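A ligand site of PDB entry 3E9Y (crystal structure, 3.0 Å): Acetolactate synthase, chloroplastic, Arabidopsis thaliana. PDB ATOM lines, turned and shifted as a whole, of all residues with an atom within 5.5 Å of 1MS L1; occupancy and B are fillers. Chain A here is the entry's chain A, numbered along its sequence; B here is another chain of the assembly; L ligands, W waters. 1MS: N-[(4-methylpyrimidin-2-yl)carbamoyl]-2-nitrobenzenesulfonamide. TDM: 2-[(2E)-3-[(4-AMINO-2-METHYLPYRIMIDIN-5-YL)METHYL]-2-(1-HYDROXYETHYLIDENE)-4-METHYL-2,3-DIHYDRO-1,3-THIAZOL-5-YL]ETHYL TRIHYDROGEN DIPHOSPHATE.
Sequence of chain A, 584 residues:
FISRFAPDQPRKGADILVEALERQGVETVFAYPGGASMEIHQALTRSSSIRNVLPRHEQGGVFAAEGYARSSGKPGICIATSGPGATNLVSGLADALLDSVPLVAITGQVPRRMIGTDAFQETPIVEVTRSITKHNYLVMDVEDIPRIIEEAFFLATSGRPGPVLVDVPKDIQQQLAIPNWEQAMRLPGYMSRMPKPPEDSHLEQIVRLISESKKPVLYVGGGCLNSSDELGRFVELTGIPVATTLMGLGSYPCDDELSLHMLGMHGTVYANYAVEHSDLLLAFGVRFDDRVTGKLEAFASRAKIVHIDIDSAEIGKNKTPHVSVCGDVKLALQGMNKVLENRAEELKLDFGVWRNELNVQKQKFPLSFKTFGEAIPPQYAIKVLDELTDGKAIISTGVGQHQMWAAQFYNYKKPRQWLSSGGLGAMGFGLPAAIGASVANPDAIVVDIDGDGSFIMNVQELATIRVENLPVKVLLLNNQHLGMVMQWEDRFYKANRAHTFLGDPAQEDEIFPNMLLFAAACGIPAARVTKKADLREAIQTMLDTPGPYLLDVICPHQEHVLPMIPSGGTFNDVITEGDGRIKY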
ATOM      1  N   ASP A 290      23.213 -29.274 -20.342  1.00  0.00           N
ATOM      2  CA  ASP A 290      21.943 -29.914 -19.971  1.00  0.00           C
ATOM      3  C   ASP A 290      20.848 -29.876 -21.061  1.00  0.00           C
ATOM      4  O   ASP A 290      19.997 -30.758 -21.117  1.00  0.00           O
ATOM      5  CB  ASP A 290      21.416 -29.343 -18.653  1.00  0.00           C
ATOM      6  CG  ASP A 290      20.904 -27.915 -18.771  1.00  0.00           C
ATOM      7  OD1 ASP A 290      21.733 -26.972 -18.756  1.00  0.00           O
ATOM      8  OD2 ASP A 290      19.678 -27.733 -18.883  1.00  0.00           O
ATOM      9  N   ARG A 291      20.894 -28.849 -21.917  1.00  0.00           N
ATOM     10  CA  ARG A 291      19.924 -28.702 -23.005  1.00  0.00           C
ATOM     11  C   ARG A 291      20.002 -29.819 -24.046  1.00  0.00           C
ATOM     12  O   ARG A 291      18.993 -30.120 -24.697  1.00  0.00           O
ATOM     13  CB  ARG A 291      20.088 -27.344 -23.700  1.00  0.00           C
ATOM     14  CG  ARG A 291      19.018 -26.331 -23.327  1.00  0.00           C
ATOM     15  CD  ARG A 291      18.819 -26.252 -21.836  1.00  0.00           C
ATOM     16  NE  ARG A 291      17.434 -25.983 -21.498  1.00  0.00           N
ATOM     17  CZ  ARG A 291      16.898 -26.130 -20.290  1.00  0.00           C
ATOM     18  NH1 ARG A 291      17.636 -26.552 -19.270  1.00  0.00           N
ATOM     19  NH2 ARG A 291      15.615 -25.857 -20.101  1.00  0.00           N
ATOM     20  N   MET A 484       8.144 -18.537 -25.761  1.00  0.00           N
ATOM     21  CA  MET A 484       8.810 -19.649 -25.098  1.00  0.00           C
ATOM     22  C   MET A 484       8.243 -19.899 -23.710  1.00  0.00           C
ATOM     23  O   MET A 484       8.056 -21.052 -23.300  1.00  0.00           O
ATOM     24  CB  MET A 484      10.320 -19.417 -25.042  1.00  0.00           C
ATOM     25  CG  MET A 484      11.131 -20.635 -24.608  1.00  0.00           C
ATOM     26  SD  MET A 484      10.847 -22.083 -25.659  1.00  0.00           S
ATOM     27  CE  MET A 484      11.959 -21.729 -27.014  1.00  0.00           C
ATOM     28  N   VAL A 485       7.966 -18.812 -22.980  1.00  0.00           N
ATOM     29  CA  VAL A 485       7.377 -18.893 -21.646  1.00  0.00           C
ATOM     30  C   VAL A 485       5.936 -19.372 -21.756  1.00  0.00           C
ATOM     31  O   VAL A 485       5.475 -20.181 -20.937  1.00  0.00           O
ATOM     32  CB  VAL A 485       7.443 -17.538 -20.909  1.00  0.00           C
ATOM     33  CG1 VAL A 485       7.111 -17.707 -19.436  1.00  0.00           C
ATOM     34  CG2 VAL A 485       8.832 -16.914 -21.058  1.00  0.00           C
ATOM     35  N   TRP A 488       5.644 -23.251 -22.327  1.00  0.00           N
ATOM     36  CA  TRP A 488       5.802 -23.933 -21.048  1.00  0.00           C
ATOM     37  C   TRP A 488       4.578 -23.739 -20.160  1.00  0.00           C
ATOM     38  O   TRP A 488       4.178 -24.639 -19.412  1.00  0.00           O
ATOM     39  CB  TRP A 488       7.067 -23.443 -20.343  1.00  0.00           C
ATOM     40  CG  TRP A 488       8.284 -24.153 -20.796  1.00  0.00           C
ATOM     41  CD1 TRP A 488       8.837 -24.129 -22.053  1.00  0.00           C
ATOM     42  CD2 TRP A 488       9.118 -25.005 -20.003  1.00  0.00           C
ATOM     43  NE1 TRP A 488       9.973 -24.918 -22.083  1.00  0.00           N
ATOM     44  CE2 TRP A 488      10.166 -25.461 -20.841  1.00  0.00           C
ATOM     45  CE3 TRP A 488       9.095 -25.430 -18.669  1.00  0.00           C
ATOM     46  CZ2 TRP A 488      11.174 -26.323 -20.376  1.00  0.00           C
ATOM     47  CZ3 TRP A 488      10.091 -26.280 -18.207  1.00  0.00           C
ATOM     48  CH2 TRP A 488      11.114 -26.723 -19.068  1.00  0.00           C
ATOM     49  N   SER A 567      12.403 -30.697 -19.483  1.00  0.00           N
ATOM     50  CA  SER A 567      13.700 -30.483 -18.832  1.00  0.00           C
ATOM     51  C   SER A 567      14.069 -31.555 -17.800  1.00  0.00           C
ATOM     52  O   SER A 567      13.276 -31.869 -16.910  1.00  0.00           O
ATOM     53  CB  SER A 567      13.762 -29.092 -18.203  1.00  0.00           C
ATOM     54  OG  SER A 567      15.095 -28.771 -17.827  1.00  0.00           O
ATOM     55  N   GLY A 568      15.278 -32.097 -17.947  1.00  0.00           N
ATOM     56  CA  GLY A 568      15.751 -33.198 -17.121  1.00  0.00           C
ATOM     57  C   GLY A 568      15.168 -34.543 -17.519  1.00  0.00           C
ATOM     58  O   GLY A 568      15.007 -35.440 -16.677  1.00  0.00           O
ATOM     59  N   GLY B  34      10.462 -15.454 -16.821  1.00  0.00           N
ATOM     60  CA  GLY B  34      11.412 -16.302 -17.512  1.00  0.00           C
ATOM     61  C   GLY B  34      11.421 -17.700 -16.922  1.00  0.00           C
ATOM     62  O   GLY B  34      10.738 -17.965 -15.924  1.00  0.00           O
ATOM     63  N   GLY B  35      12.200 -18.583 -17.521  1.00  0.00           N
ATOM     64  CA  GLY B  35      12.268 -19.986 -17.127  1.00  0.00           C
ATOM     65  C   GLY B  35      12.379 -20.247 -15.636  1.00  0.00           C
ATOM     66  O   GLY B  35      11.600 -21.017 -15.074  1.00  0.00           O
ATOM     67  N   ALA B  36      13.335 -19.578 -15.000  1.00  0.00           N
ATOM     68  CA  ALA B  36      13.671 -19.815 -13.592  1.00  0.00           C
ATOM     69  C   ALA B  36      12.793 -19.087 -12.570  1.00  0.00           C
ATOM     70  O   ALA B  36      12.957 -19.283 -11.360  1.00  0.00           O
ATOM     71  CB  ALA B  36      15.141 -19.515 -13.339  1.00  0.00           C
ATOM     72  N   MET B  38       9.208 -18.581 -13.420  1.00  0.00           N
ATOM     73  CA  MET B  38       7.820 -18.877 -13.807  1.00  0.00           C
ATOM     74  C   MET B  38       6.907 -19.146 -12.612  1.00  0.00           C
ATOM     75  O   MET B  38       5.815 -18.596 -12.528  1.00  0.00           O
ATOM     76  CB  MET B  38       7.755 -20.076 -14.755  1.00  0.00           C
ATOM     77  CG  MET B  38       8.168 -19.767 -16.187  1.00  0.00           C
ATOM     78  SD  MET B  38       7.620 -21.064 -17.309  1.00  0.00           S
ATOM     79  CE  MET B  38       5.871 -20.678 -17.424  1.00  0.00           C
ATOM     80  N   SER B  82      16.556 -16.043 -13.878  1.00  0.00           N
ATOM     81  CA  SER B  82      17.987 -16.289 -13.759  1.00  0.00           C
ATOM     82  C   SER B  82      18.744 -15.686 -14.936  1.00  0.00           C
ATOM     83  O   SER B  82      18.147 -15.165 -15.880  1.00  0.00           O
ATOM     84  CB  SER B  82      18.251 -17.781 -13.700  1.00  0.00           C
ATOM     85  OG  SER B  82      17.896 -18.392 -14.937  1.00  0.00           O
ATOM     86  N   GLN B 109      16.669 -18.723  -9.889  1.00  0.00           N
ATOM     87  CA  GLN B 109      17.981 -19.306 -10.118  1.00  0.00           C
ATOM     88  C   GLN B 109      17.784 -20.741 -10.582  1.00  0.00           C
ATOM     89  O   GLN B 109      16.719 -21.329 -10.358  1.00  0.00           O
ATOM     90  CB  GLN B 109      18.799 -19.251  -8.821  1.00  0.00           C
ATOM     91  CG  GLN B 109      20.181 -19.883  -8.876  1.00  0.00           C
ATOM     92  CD  GLN B 109      21.082 -19.229  -9.888  1.00  0.00           C
ATOM     93  OE1 GLN B 109      21.023 -19.530 -11.081  1.00  0.00           O
ATOM     94  NE2 GLN B 109      21.935 -18.312  -9.421  1.00  0.00           N
ATOM     95  N   VAL B 110      18.800 -21.300 -11.239  1.00  0.00           N
ATOM     96  CA  VAL B 110      18.798 -22.712 -11.613  1.00  0.00           C
ATOM     97  C   VAL B 110      18.609 -23.578 -10.359  1.00  0.00           C
ATOM     98  O   VAL B 110      18.901 -23.116  -9.234  1.00  0.00           O
ATOM     99  CB  VAL B 110      20.108 -23.112 -12.326  1.00  0.00           C
ATOM    100  CG1 VAL B 110      20.338 -22.234 -13.555  1.00  0.00           C
ATOM    101  CG2 VAL B 110      21.297 -23.042 -11.375  1.00  0.00           C
ATOM    102  N   PRO B 111      18.105 -24.819 -10.520  1.00  0.00           N
ATOM    103  CA  PRO B 111      17.944 -25.705  -9.356  1.00  0.00           C
ATOM    104  C   PRO B 111      19.279 -25.932  -8.639  1.00  0.00           C
ATOM    105  O   PRO B 111      20.325 -26.002  -9.294  1.00  0.00           O
ATOM    106  CB  PRO B 111      17.451 -27.002  -9.968  1.00  0.00           C
ATOM    107  CG  PRO B 111      16.843 -26.618 -11.266  1.00  0.00           C
ATOM    108  CD  PRO B 111      17.656 -25.477 -11.759  1.00  0.00           C
ATOM    109  N   MET B 114      22.465 -27.783  -9.563  1.00  0.00           N
ATOM    110  CA  MET B 114      23.177 -27.345 -10.756  1.00  0.00           C
ATOM    111  C   MET B 114      23.932 -26.031 -10.603  1.00  0.00           C
ATOM    112  O   MET B 114      24.574 -25.564 -11.547  1.00  0.00           O
ATOM    113  CB  MET B 114      22.198 -27.245 -11.934  1.00  0.00           C
ATOM    114  CG  MET B 114      21.443 -28.534 -12.179  1.00  0.00           C
ATOM    115  SD  MET B 114      20.385 -28.429 -13.630  1.00  0.00           S
ATOM    116  CE  MET B 114      21.618 -28.541 -14.939  1.00  0.00           C
ATOM    117  N   ALA B 119      25.048 -23.998 -15.938  1.00  0.00           N
ATOM    118  CA  ALA B 119      23.809 -24.518 -16.486  1.00  0.00           C
ATOM    119  C   ALA B 119      23.099 -23.479 -17.371  1.00  0.00           C
ATOM    120  O   ALA B 119      23.530 -22.332 -17.477  1.00  0.00           O
ATOM    121  CB  ALA B 119      22.884 -24.988 -15.373  1.00  0.00           C
ATOM    122  N   PHE B 120      22.012 -23.917 -18.013  1.00  0.00           N
ATOM    123  CA  PHE B 120      21.211 -23.048 -18.860  1.00  0.00           C
ATOM    124  C   PHE B 120      20.742 -21.820 -18.088  1.00  0.00           C
ATOM    125  O   PHE B 120      20.036 -21.940 -17.074  1.00  0.00           O
ATOM    126  CB  PHE B 120      20.015 -23.826 -19.416  1.00  0.00           C
ATOM    127  CG  PHE B 120      19.109 -23.014 -20.307  1.00  0.00           C
ATOM    128  CD1 PHE B 120      19.566 -22.522 -21.517  1.00  0.00           C
ATOM    129  CD2 PHE B 120      17.802 -22.765 -19.925  1.00  0.00           C
ATOM    130  CE1 PHE B 120      18.736 -21.771 -22.340  1.00  0.00           C
ATOM    131  CE2 PHE B 120      16.953 -22.023 -20.739  1.00  0.00           C
ATOM    132  CZ  PHE B 120      17.419 -21.525 -21.957  1.00  0.00           C
ATOM    133  N   GLN B 121      21.153 -20.648 -18.574  1.00  0.00           N
ATOM    134  CA  GLN B 121      20.824 -19.352 -17.964  1.00  0.00           C
ATOM    135  C   GLN B 121      21.316 -19.232 -16.518  1.00  0.00           C
ATOM    136  O   GLN B 121      20.597 -18.726 -15.658  1.00  0.00           O
ATOM    137  CB  GLN B 121      19.327 -19.062 -18.053  1.00  0.00           C
ATOM    138  CG  GLN B 121      18.758 -19.128 -19.450  1.00  0.00           C
ATOM    139  CD  GLN B 121      17.415 -18.438 -19.581  1.00  0.00           C
ATOM    140  OE1 GLN B 121      16.470 -18.762 -18.865  1.00  0.00           O
ATOM    141  NE2 GLN B 121      17.336 -17.484 -20.512  1.00  0.00           N
ATOM    142  N   LYS B 170      15.003 -22.763  -8.579  1.00  0.00           N
ATOM    143  CA  LYS B 170      13.741 -23.264  -9.124  1.00  0.00           C
ATOM    144  C   LYS B 170      13.131 -24.399  -8.300  1.00  0.00           C
ATOM    145  O   LYS B 170      11.921 -24.418  -8.062  1.00  0.00           O
ATOM    146  CB  LYS B 170      13.904 -23.667 -10.592  1.00  0.00           C
ATOM    147  CG  LYS B 170      12.657 -24.289 -11.207  1.00  0.00           C
ATOM    148  CD  LYS B 170      12.489 -23.922 -12.667  1.00  0.00           C
ATOM    149  CE  LYS B 170      11.289 -24.638 -13.279  1.00  0.00           C
ATOM    150  NZ  LYS B 170      10.911 -24.058 -14.609  1.00  0.00           N
HETATM  151  O8  1MS L   1      16.409 -21.984 -15.325  1.00  0.00           O
HETATM  152  N7  1MS L   1      15.905 -23.311 -15.252  1.00  0.00           N
HETATM  153  O9  1MS L   1      14.540 -23.466 -14.932  1.00  0.00           O
HETATM  154  C1  1MS L   1      16.734 -24.347 -15.476  1.00  0.00           C
HETATM  155  C6  1MS L   1      18.054 -24.026 -15.763  1.00  0.00           C
HETATM  156  C5  1MS L   1      19.037 -24.967 -16.025  1.00  0.00           C
HETATM  157  C4  1MS L   1      18.822 -26.353 -16.029  1.00  0.00           C
HETATM  158  C3  1MS L   1      17.398 -26.826 -15.715  1.00  0.00           C
HETATM  159  C2  1MS L   1      16.384 -25.707 -15.452  1.00  0.00           C
HETATM  160  S10 1MS L   1      14.758 -26.288 -15.088  1.00  0.00           S
HETATM  161  O11 1MS L   1      14.644 -27.715 -15.513  1.00  0.00           O
HETATM  162  O12 1MS L   1      14.540 -26.224 -13.615  1.00  0.00           O
HETATM  163  N13 1MS L   1      13.532 -25.446 -15.830  1.00  0.00           N
HETATM  164  C14 1MS L   1      13.648 -25.138 -17.137  1.00  0.00           C
HETATM  165  O15 1MS L   1      14.482 -25.670 -17.865  1.00  0.00           O
HETATM  166  N16 1MS L   1      12.775 -24.212 -17.546  1.00  0.00           N
HETATM  167  C18 1MS L   1      12.660 -23.715 -18.796  1.00  0.00           C
HETATM  168  N17 1MS L   1      13.530 -24.020 -19.781  1.00  0.00           N
HETATM  169  C23 1MS L   1      13.416 -23.517 -21.003  1.00  0.00           C
HETATM  170  C22 1MS L   1      12.383 -22.632 -21.327  1.00  0.00           C
HETATM  171  C20 1MS L   1      11.466 -22.293 -20.348  1.00  0.00           C
HETATM  172  C21 1MS L   1      10.427 -21.415 -20.627  1.00  0.00           C
HETATM  173  N19 1MS L   1      11.601 -22.829 -19.055  1.00  0.00           N
HETATM  174  O1A TDM L   2       8.668 -12.566 -28.380  1.00  0.00           O
HETATM  175  PA  TDM L   2       9.930 -13.169 -27.874  1.00  0.00           P
HETATM  176  O2A TDM L   2      11.151 -12.198 -28.152  1.00  0.00           O
HETATM  177  O3A TDM L   2      10.325 -14.553 -28.628  1.00  0.00           O
HETATM  178  PB  TDM L   2       9.294 -15.735 -28.935  1.00  0.00           P
HETATM  179  O2B TDM L   2       9.446 -16.275 -30.311  1.00  0.00           O
HETATM  180  O3B TDM L   2       9.529 -16.881 -27.819  1.00  0.00           O
HETATM  181  O1B TDM L   2       7.792 -15.215 -28.666  1.00  0.00           O
HETATM  182  O7  TDM L   2       9.948 -13.443 -26.291  1.00  0.00           O
HETATM  183  C7  TDM L   2      10.964 -14.226 -25.655  1.00  0.00           C
HETATM  184  C6  TDM L   2      10.318 -15.015 -24.523  1.00  0.00           C
HETATM  185  C5  TDM L   2      11.315 -15.527 -23.486  1.00  0.00           C
HETATM  186  S1  TDM L   2      12.200 -16.979 -23.766  1.00  0.00           S
HETATM  187  C2  TDM L   2      13.049 -16.968 -22.273  1.00  0.00           C
HETATM  188  C27 TDM L   2      13.931 -17.895 -21.878  1.00  0.00           C
HETATM  189  C29 TDM L   2      14.257 -19.099 -22.766  1.00  0.00           C
HETATM  190  O28 TDM L   2      14.639 -17.769 -20.527  1.00  0.00           O
HETATM  191  N3  TDM L   2      12.579 -15.694 -21.531  1.00  0.00           N
HETATM  192  C4  TDM L   2      11.663 -14.987 -22.235  1.00  0.00           C
HETATM  193  CM4 TDM L   2      11.042 -13.689 -21.717  1.00  0.00           C
HETATM  194  C7' TDM L   2      13.107 -15.291 -20.208  1.00  0.00           C
HETATM  195  C5' TDM L   2      14.119 -14.141 -20.427  1.00  0.00           C
HETATM  196  C4' TDM L   2      15.275 -14.198 -21.226  1.00  0.00           C
HETATM  197  N4' TDM L   2      15.610 -15.304 -21.881  1.00  0.00           N
HETATM  198  N3' TDM L   2      16.072 -13.119 -21.345  1.00  0.00           N
HETATM  199  C2' TDM L   2      15.780 -11.972 -20.706  1.00  0.00           C
HETATM  200  CM2 TDM L   2      16.706 -10.768 -20.862  1.00  0.00           C
HETATM  201  N1' TDM L   2      14.679 -11.890 -19.937  1.00  0.00           N
HETATM  202  C6' TDM L   2      13.866 -12.921 -19.783  1.00  0.00           C
HETATM  203  O   HOH W   1      13.828 -28.364 -11.353  1.00  0.00           O
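O15 of 1MS L1 is in hydrogen-bond range of NH2 of Arg 291 (2.5 Å). OG of Ser 567 is in hydrogen-bond range of O11 of 1MS L1. A nitrogen (N13) of 1MS L1 is in hydrogen-bond range of the side-chain amino group of Lys 170 of chain B, at 3.2 Å. O3B of TDM L2 is in hydrogen-bond range of N of Met 484 (3.0 Å). O28 of TDM L2 sits at hydrogen-bond distance from OE1 of Gln 121 of chain B.
The guanidinium group (NE) of Arg 291 lies within salt-bridge range of the side-chain carboxylate (OD2) of Asp 290. The side-chain amino group (NZ) of Lys 170 of chain B is in hydrogen-bond range of the backbone carbonyl oxygen (O) of Gly 35 of chain B. N of Phe 120 of chain B sits at hydrogen-bond distance from OD1 of Asp 290, 3.2 Å away. OG of Ser 82 of chain B is in hydrogen-bond range of O of Gln 121 of chain B.
Asp 290 touches 1MS L1 (OD2 to C4, 3.3 Å). O of Met 484 touches C21 of 1MS L1 (3.6 Å). Trp 488 touches 1MS L1 (CZ2 to N17, 3.3 Å). Gly 35 of chain B touches 1MS L1. CB of Ala 36 of chain B touches O8 of 1MS L1, at 3.4 Å. OG of Ser 82 of chain B touches O8 of 1MS L1, at 3.9 Å. CG1 of Val 110 of chain B touches C6 of 1MS L1, 3.6 Å away. CG of Pro 111 of chain B touches O12 of 1MS L1, 3.3 Å away. Met 114 of chain B touches 1MS L1 (SD to C4, 3.5 Å). Ala 119 of chain B touches 1MS L1. O of Phe 120 of chain B touches C6 of 1MS L1, 3.2 Å away. Hydrophobic or aromatic side chains within 4 Å of 1MS L1: Trp 488, Ala 36 of chain B, Val 110 of chain B, Pro 111 of chain B, Met 114 of chain B, Ala 119 of chain B and Phe 120 of chain B. Of the 20 residues printed, 14 come within 4 Å of 1MS L1.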
